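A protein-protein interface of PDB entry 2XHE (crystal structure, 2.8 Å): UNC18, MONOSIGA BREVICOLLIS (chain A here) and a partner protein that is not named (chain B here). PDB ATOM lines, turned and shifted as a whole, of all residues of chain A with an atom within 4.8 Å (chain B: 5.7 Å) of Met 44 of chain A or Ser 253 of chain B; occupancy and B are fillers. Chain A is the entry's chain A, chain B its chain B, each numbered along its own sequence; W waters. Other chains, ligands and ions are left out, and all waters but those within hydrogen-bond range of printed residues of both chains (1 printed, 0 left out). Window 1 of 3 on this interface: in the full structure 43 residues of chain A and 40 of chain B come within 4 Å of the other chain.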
ATOM      1  N   ALA A  42      -4.002  16.140 -23.601  1.00  0.00           N
ATOM      2  CA  ALA A  42      -4.324  16.140 -22.174  1.00  0.00           C
ATOM      3  C   ALA A  42      -5.201  17.316 -21.750  1.00  0.00           C
ATOM      4  O   ALA A  42      -4.919  18.454 -22.106  1.00  0.00           O
ATOM      5  CB  ALA A  42      -3.030  16.147 -21.357  1.00  0.00           C
ATOM      6  N   ARG A  43      -6.241  17.046 -20.964  1.00  0.00           N
ATOM      7  CA  ARG A  43      -7.045  18.114 -20.369  1.00  0.00           C
ATOM      8  C   ARG A  43      -6.279  18.732 -19.193  1.00  0.00           C
ATOM      9  O   ARG A  43      -5.224  18.226 -18.815  1.00  0.00           O
ATOM     10  CB  ARG A  43      -8.392  17.564 -19.894  1.00  0.00           C
ATOM     11  CG  ARG A  43      -9.129  16.692 -20.902  1.00  0.00           C
ATOM     12  CD  ARG A  43      -9.629  17.503 -22.095  1.00  0.00           C
ATOM     13  NE  ARG A  43      -9.191  16.936 -23.374  1.00  0.00           N
ATOM     14  CZ  ARG A  43      -8.139  17.373 -24.066  1.00  0.00           C
ATOM     15  NH1 ARG A  43      -7.417  18.390 -23.605  1.00  0.00           N
ATOM     16  NH2 ARG A  43      -7.804  16.799 -25.215  1.00  0.00           N
ATOM     17  N   MET A  44      -6.791  19.820 -18.615  1.00  0.00           N
ATOM     18  CA  MET A  44      -6.175  20.405 -17.412  1.00  0.00           C
ATOM     19  C   MET A  44      -6.290  19.474 -16.196  1.00  0.00           C
ATOM     20  O   MET A  44      -5.370  19.354 -15.400  1.00  0.00           O
ATOM     21  CB  MET A  44      -6.782  21.770 -17.069  1.00  0.00           C
ATOM     22  CG  MET A  44      -5.881  22.969 -17.375  1.00  0.00           C
ATOM     23  SD  MET A  44      -4.314  22.958 -16.477  1.00  0.00           S
ATOM     24  CE  MET A  44      -3.722  24.632 -16.740  1.00  0.00           C
ATOM     25  N   SER A  45      -7.442  18.836 -16.070  1.00  0.00           N
ATOM     26  CA  SER A  45      -7.715  17.897 -15.005  1.00  0.00           C
ATOM     27  C   SER A  45      -6.705  16.741 -15.016  1.00  0.00           C
ATOM     28  O   SER A  45      -6.346  16.225 -13.965  1.00  0.00           O
ATOM     29  CB  SER A  45      -9.153  17.375 -15.151  1.00  0.00           C
ATOM     30  OG  SER A  45      -9.509  16.481 -14.112  1.00  0.00           O
ATOM     31  N   GLU A  46      -6.253  16.335 -16.202  1.00  0.00           N
ATOM     32  CA  GLU A  46      -5.303  15.227 -16.324  1.00  0.00           C
ATOM     33  C   GLU A  46      -3.885  15.693 -16.034  1.00  0.00           C
ATOM     34  O   GLU A  46      -3.002  14.887 -15.777  1.00  0.00           O
ATOM     35  CB  GLU A  46      -5.358  14.606 -17.727  1.00  0.00           C
ATOM     36  CG  GLU A  46      -6.517  13.652 -17.953  1.00  0.00           C
ATOM     37  CD  GLU A  46      -6.628  13.183 -19.395  1.00  0.00           C
ATOM     38  OE1 GLU A  46      -6.310  13.971 -20.319  1.00  0.00           O
ATOM     39  OE2 GLU A  46      -7.049  12.023 -19.606  1.00  0.00           O
ATOM     40  N   ILE A  47      -3.681  17.003 -16.095  1.00  0.00           N
ATOM     41  CA  ILE A  47      -2.378  17.604 -15.858  1.00  0.00           C
ATOM     42  C   ILE A  47      -2.229  17.848 -14.355  1.00  0.00           C
ATOM     43  O   ILE A  47      -1.142  17.716 -13.780  1.00  0.00           O
ATOM     44  CB  ILE A  47      -2.224  18.928 -16.677  1.00  0.00           C
ATOM     45  CG1 ILE A  47      -0.933  18.929 -17.480  1.00  0.00           C
ATOM     46  CG2 ILE A  47      -2.299  20.157 -15.794  1.00  0.00           C
ATOM     47  CD1 ILE A  47      -1.033  18.123 -18.740  1.00  0.00           C
ATOM     48  N   LEU A  48      -3.348  18.194 -13.726  1.00  0.00           N
ATOM     49  CA  LEU A  48      -3.388  18.483 -12.304  1.00  0.00           C
ATOM     50  C   LEU A  48      -2.985  17.253 -11.531  1.00  0.00           C
ATOM     51  O   LEU A  48      -2.098  17.299 -10.687  1.00  0.00           O
ATOM     52  CB  LEU A  48      -4.796  18.893 -11.892  1.00  0.00           C
ATOM     53  CG  LEU A  48      -4.931  20.274 -11.257  1.00  0.00           C
ATOM     54  CD1 LEU A  48      -3.757  21.162 -11.637  1.00  0.00           C
ATOM     55  CD2 LEU A  48      -6.268  20.913 -11.648  1.00  0.00           C
ATOM     56  N   VAL A  55       0.189  25.684 -15.805  1.00  0.00           N
ATOM     57  CA  VAL A  55       0.914  25.705 -17.060  1.00  0.00           C
ATOM     58  C   VAL A  55       1.185  27.170 -17.426  1.00  0.00           C
ATOM     59  O   VAL A  55       0.306  28.029 -17.307  1.00  0.00           O
ATOM     60  CB  VAL A  55       0.117  24.996 -18.153  1.00  0.00           C
ATOM     61  CG1 VAL A  55       0.991  24.736 -19.400  1.00  0.00           C
ATOM     62  CG2 VAL A  55      -0.464  23.704 -17.594  1.00  0.00           C
ATOM     63  N   ARG B 134      -5.556  31.740 -11.030  1.00  0.00           N
ATOM     64  CA  ARG B 134      -5.584  30.726 -12.080  1.00  0.00           C
ATOM     65  C   ARG B 134      -5.499  29.315 -11.495  1.00  0.00           C
ATOM     66  O   ARG B 134      -6.316  28.449 -11.830  1.00  0.00           O
ATOM     67  CB  ARG B 134      -4.453  30.955 -13.081  1.00  0.00           C
ATOM     68  CG  ARG B 134      -4.671  32.139 -14.022  1.00  0.00           C
ATOM     69  CD  ARG B 134      -3.447  32.364 -14.900  1.00  0.00           C
ATOM     70  NE  ARG B 134      -3.045  31.130 -15.567  1.00  0.00           N
ATOM     71  CZ  ARG B 134      -1.787  30.813 -15.855  1.00  0.00           C
ATOM     72  NH1 ARG B 134      -0.802  31.641 -15.531  1.00  0.00           N
ATOM     73  NH2 ARG B 134      -1.516  29.662 -16.456  1.00  0.00           N
ATOM     74  N   SER B 138      -8.399  26.275 -11.517  1.00  0.00           N
ATOM     75  CA  SER B 138      -8.240  24.944 -12.103  1.00  0.00           C
ATOM     76  C   SER B 138      -8.340  23.830 -11.064  1.00  0.00           C
ATOM     77  O   SER B 138      -8.881  22.764 -11.354  1.00  0.00           O
ATOM     78  CB  SER B 138      -6.962  24.823 -12.931  1.00  0.00           C
ATOM     79  OG  SER B 138      -5.859  25.350 -12.240  1.00  0.00           O
ATOM     80  N   SER B 142     -11.409  21.109 -11.396  1.00  0.00           N
ATOM     81  CA  SER B 142     -11.012  19.716 -11.515  1.00  0.00           C
ATOM     82  C   SER B 142     -11.605  18.831 -10.403  1.00  0.00           C
ATOM     83  O   SER B 142     -12.145  17.754 -10.676  1.00  0.00           O
ATOM     84  CB  SER B 142      -9.490  19.615 -11.537  1.00  0.00           C
ATOM     85  OG  SER B 142      -9.078  18.272 -11.723  1.00  0.00           O
ATOM     86  N   ILE B 247     -12.727  25.683 -18.991  1.00  0.00           N
ATOM     87  CA  ILE B 247     -11.582  25.696 -18.071  1.00  0.00           C
ATOM     88  C   ILE B 247     -10.713  24.425 -18.112  1.00  0.00           C
ATOM     89  O   ILE B 247      -9.501  24.489 -17.876  1.00  0.00           O
ATOM     90  CB  ILE B 247     -12.012  26.016 -16.605  1.00  0.00           C
ATOM     91  CG1 ILE B 247     -10.795  26.049 -15.669  1.00  0.00           C
ATOM     92  CG2 ILE B 247     -13.044  25.013 -16.107  1.00  0.00           C
ATOM     93  CD1 ILE B 247     -10.997  26.907 -14.429  1.00  0.00           C
ATOM     94  N   ASP B 248     -11.322  23.281 -18.412  1.00  0.00           N
ATOM     95  CA  ASP B 248     -10.559  22.049 -18.565  1.00  0.00           C
ATOM     96  C   ASP B 248      -9.627  22.065 -19.780  1.00  0.00           C
ATOM     97  O   ASP B 248      -8.880  21.115 -20.005  1.00  0.00           O
ATOM     98  CB  ASP B 248     -11.481  20.831 -18.636  1.00  0.00           C
ATOM     99  CG  ASP B 248     -10.809  19.567 -18.112  1.00  0.00           C
ATOM    100  OD1 ASP B 248      -9.893  19.696 -17.268  1.00  0.00           O
ATOM    101  OD2 ASP B 248     -11.194  18.452 -18.533  1.00  0.00           O
ATOM    102  N   ARG B 249      -9.676  23.133 -20.567  1.00  0.00           N
ATOM    103  CA  ARG B 249      -8.816  23.255 -21.742  1.00  0.00           C
ATOM    104  C   ARG B 249      -7.532  23.980 -21.372  1.00  0.00           C
ATOM    105  O   ARG B 249      -7.581  25.060 -20.779  1.00  0.00           O
ATOM    106  CB  ARG B 249      -9.559  23.974 -22.872  1.00  0.00           C
ATOM    107  CG  ARG B 249     -10.293  23.028 -23.820  1.00  0.00           C
ATOM    108  CD  ARG B 249      -9.301  22.269 -24.705  1.00  0.00           C
ATOM    109  NE  ARG B 249      -9.836  20.997 -25.191  1.00  0.00           N
ATOM    110  CZ  ARG B 249      -9.191  20.197 -26.039  1.00  0.00           C
ATOM    111  NH1 ARG B 249      -7.987  20.540 -26.494  1.00  0.00           N
ATOM    112  NH2 ARG B 249      -9.749  19.057 -26.436  1.00  0.00           N
ATOM    113  N   ILE B 250      -6.384  23.378 -21.687  1.00  0.00           N
ATOM    114  CA  ILE B 250      -5.104  23.945 -21.252  1.00  0.00           C
ATOM    115  C   ILE B 250      -4.913  25.302 -21.898  1.00  0.00           C
ATOM    116  O   ILE B 250      -4.750  26.312 -21.211  1.00  0.00           O
ATOM    117  CB  ILE B 250      -3.889  23.063 -21.595  1.00  0.00           C
ATOM    118  CG1 ILE B 250      -4.019  21.668 -20.992  1.00  0.00           C
ATOM    119  CG2 ILE B 250      -2.618  23.683 -21.059  1.00  0.00           C
ATOM    120  CD1 ILE B 250      -2.846  20.767 -21.335  1.00  0.00           C
ATOM    121  N   GLU B 251      -4.956  25.316 -23.228  1.00  0.00           N
ATOM    122  CA  GLU B 251      -4.838  26.550 -23.993  1.00  0.00           C
ATOM    123  C   GLU B 251      -5.595  27.707 -23.346  1.00  0.00           C
ATOM    124  O   GLU B 251      -5.117  28.834 -23.346  1.00  0.00           O
ATOM    125  CB  GLU B 251      -5.310  26.337 -25.430  1.00  0.00           C
ATOM    126  CG  GLU B 251      -4.350  25.522 -26.281  1.00  0.00           C
ATOM    127  CD  GLU B 251      -4.241  26.032 -27.715  1.00  0.00           C
ATOM    128  OE1 GLU B 251      -5.297  26.291 -28.344  1.00  0.00           O
ATOM    129  OE2 GLU B 251      -3.096  26.171 -28.215  1.00  0.00           O
ATOM    130  N   PHE B 252      -6.768  27.434 -22.784  1.00  0.00           N
ATOM    131  CA  PHE B 252      -7.566  28.505 -22.202  1.00  0.00           C
ATOM    132  C   PHE B 252      -6.901  29.094 -20.973  1.00  0.00           C
ATOM    133  O   PHE B 252      -6.832  30.314 -20.837  1.00  0.00           O
ATOM    134  CB  PHE B 252      -8.992  28.055 -21.867  1.00  0.00           C
ATOM    135  CG  PHE B 252      -9.794  29.096 -21.126  1.00  0.00           C
ATOM    136  CD1 PHE B 252     -10.139  30.295 -21.739  1.00  0.00           C
ATOM    137  CD2 PHE B 252     -10.200  28.879 -19.812  1.00  0.00           C
ATOM    138  CE1 PHE B 252     -10.875  31.261 -21.058  1.00  0.00           C
ATOM    139  CE2 PHE B 252     -10.939  29.840 -19.126  1.00  0.00           C
ATOM    140  CZ  PHE B 252     -11.277  31.033 -19.754  1.00  0.00           C
ATOM    141  N   SER B 253      -6.420  28.237 -20.075  1.00  0.00           N
ATOM    142  CA  SER B 253      -5.743  28.716 -18.869  1.00  0.00           C
ATOM    143  C   SER B 253      -4.547  29.617 -19.213  1.00  0.00           C
ATOM    144  O   SER B 253      -4.511  30.784 -18.824  1.00  0.00           O
ATOM    145  CB  SER B 253      -5.303  27.548 -17.973  1.00  0.00           C
ATOM    146  OG  SER B 253      -4.634  27.999 -16.800  1.00  0.00           O
ATOM    147  N   VAL B 254      -3.584  29.081 -19.959  1.00  0.00           N
ATOM    148  CA  VAL B 254      -2.348  29.812 -20.264  1.00  0.00           C
ATOM    149  C   VAL B 254      -2.535  31.066 -21.143  1.00  0.00           C
ATOM    150  O   VAL B 254      -1.604  31.843 -21.325  1.00  0.00           O
ATOM    151  CB  VAL B 254      -1.234  28.856 -20.793  1.00  0.00           C
ATOM    152  CG1 VAL B 254      -1.837  27.702 -21.550  1.00  0.00           C
ATOM    153  CG2 VAL B 254      -0.177  29.596 -21.621  1.00  0.00           C
ATOM    154  N   GLU B 255      -3.744  31.276 -21.657  1.00  0.00           N
ATOM    155  CA  GLU B 255      -4.063  32.502 -22.384  1.00  0.00           C
ATOM    156  C   GLU B 255      -4.327  33.660 -21.418  1.00  0.00           C
ATOM    157  O   GLU B 255      -4.028  34.812 -21.724  1.00  0.00           O
ATOM    158  CB  GLU B 255      -5.279  32.301 -23.289  1.00  0.00           C
ATOM    159  CG  GLU B 255      -5.801  33.592 -23.925  1.00  0.00           C
ATOM    160  CD  GLU B 255      -7.316  33.597 -24.122  1.00  0.00           C
ATOM    161  OE1 GLU B 255      -7.991  32.679 -23.602  1.00  0.00           O
ATOM    162  OE2 GLU B 255      -7.830  34.524 -24.788  1.00  0.00           O
ATOM    163  N   GLN B 256      -4.883  33.356 -20.251  1.00  0.00           N
ATOM    164  CA  GLN B 256      -5.161  34.395 -19.261  1.00  0.00           C
ATOM    165  C   GLN B 256      -4.026  34.593 -18.239  1.00  0.00           C
ATOM    166  O   GLN B 256      -4.279  34.871 -17.065  1.00  0.00           O
ATOM    167  CB  GLN B 256      -6.493  34.120 -18.552  1.00  0.00           C
ATOM    168  CG  GLN B 256      -6.644  32.698 -18.031  1.00  0.00           C
ATOM    169  CD  GLN B 256      -7.965  32.461 -17.325  1.00  0.00           C
ATOM    170  OE1 GLN B 256      -8.728  33.391 -17.081  1.00  0.00           O
ATOM    171  NE2 GLN B 256      -8.239  31.206 -16.990  1.00  0.00           N
ATOM    172  N   SER B 257      -2.782  34.461 -18.695  1.00  0.00           N
ATOM    173  CA  SER B 257      -1.606  34.636 -17.843  1.00  0.00           C
ATOM    174  C   SER B 257      -1.219  36.101 -17.728  1.00  0.00           C
ATOM    175  O   SER B 257      -1.605  36.911 -18.569  1.00  0.00           O
ATOM    176  CB  SER B 257      -0.427  33.874 -18.427  1.00  0.00           C
ATOM    177  OG  SER B 257      -0.876  32.694 -19.052  1.00  0.00           O
HETATM  178  O   HOH W   1      -6.236  20.879 -23.260  1.00  0.00           O
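O of Asp 248 of chain B sits at hydrogen-bond distance from N of Met 44 of chain A (2.8 Å).
The side-chain hydroxyl (OG) of Ser 142 of chain B is in hydrogen-bond range of the side-chain hydroxyl (OG) of Ser 45 of chain A.
OD1 of Asp 248 of chain B lies within hydrogen-bond range of N of Ser 45 of chain A (2.9 Å).
The backbone carbonyl oxygen (O) of Val 55 of chain A lies within hydrogen-bond range of the guanidinium group (NH2) of Arg 134 of chain B (2.6 Å).
NH2 of Arg 43 of chain A lies close to NH2 of Arg 249 of chain B (3.2 Å).
The backbone NH of Arg 43 of chain A sits at hydrogen-bond distance from the side-chain carboxylate of Glu 46 of chain A (3.1 Å).
The backbone carbonyl oxygen of Arg 134 of chain B sits at hydrogen-bond distance from the side-chain hydroxyl of Ser 138 of chain B (3.2 Å).
The backbone carbonyl oxygen of Val 254 of chain B sits at hydrogen-bond distance from the side-chain hydroxyl of Ser 257 of chain B, 2.5 Å away.
Among the printed residues, pairs that only touch across the chains: Ala 42 of chain A with Ile 250 of chain B (3.2 Å), Arg 43 of chain A with Asp 248 of chain B (3.2 Å), Met 44 of chain A with Ile 247 of chain B (3.9 Å), Met 44 of chain A with Ser 253 of chain B (3.5 Å), Leu 48 of chain A with Ser 138 of chain B (3.2 Å), Leu 48 of chain A with Ser 142 of chain B (3.5 Å) and Val 55 of chain A with Val 254 of chain B (3.9 Å).
Printed residues of chain B within 4 Å of Arg 43 of chain A: Asp 248 (3.2 Å) and Arg 249 (3.2 Å).
Met 44 of chain A touches just these residues of chain B: Ile 247 (3.9 Å), Asp 248 (2.8 Å) and Ser 253 (3.5 Å).
Of the printed residues of chain B, Leu 48 of chain A touches Ser 138 and Ser 142.
Printed residues of chain A within 4 Å of Ile 250 of chain B: Ala 42.
Phe 252 of chain B touches none of the printed residues of chain A.
Ser 253 of chain B touches just one residue of chain A: Met 44 (3.5 Å).
Hydrophobic or aromatic side chains of chain B within 4 Å of the printed part of chain A: Ile 250 and Val 254.
Along chain B the printed residues that touch a printed residue of chain A span positions 134 to 254.
Of the 8 printed residues of chain A, 6 touch a printed residue of chain B.
Hydrophobic or aromatic side chains of chain A within 4 Å of the printed part of chain B: Met 44 and Leu 48.
Among the printed residues, 12 pairs touch across the chains.
Among the printed residues, no Asp or Glu carboxylate lies within 4 Å of a Lys or Arg side-chain nitrogen of the other chain.
Water W1 lies within hydrogen-bond range of the guanidinium group of Arg 43 of chain A (2.8 Å), the backbone NH of Ile 250 of chain B (3.0 Å) and the backbone carbonyl oxygen of Ala 42 of chain A (3.0 Å).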
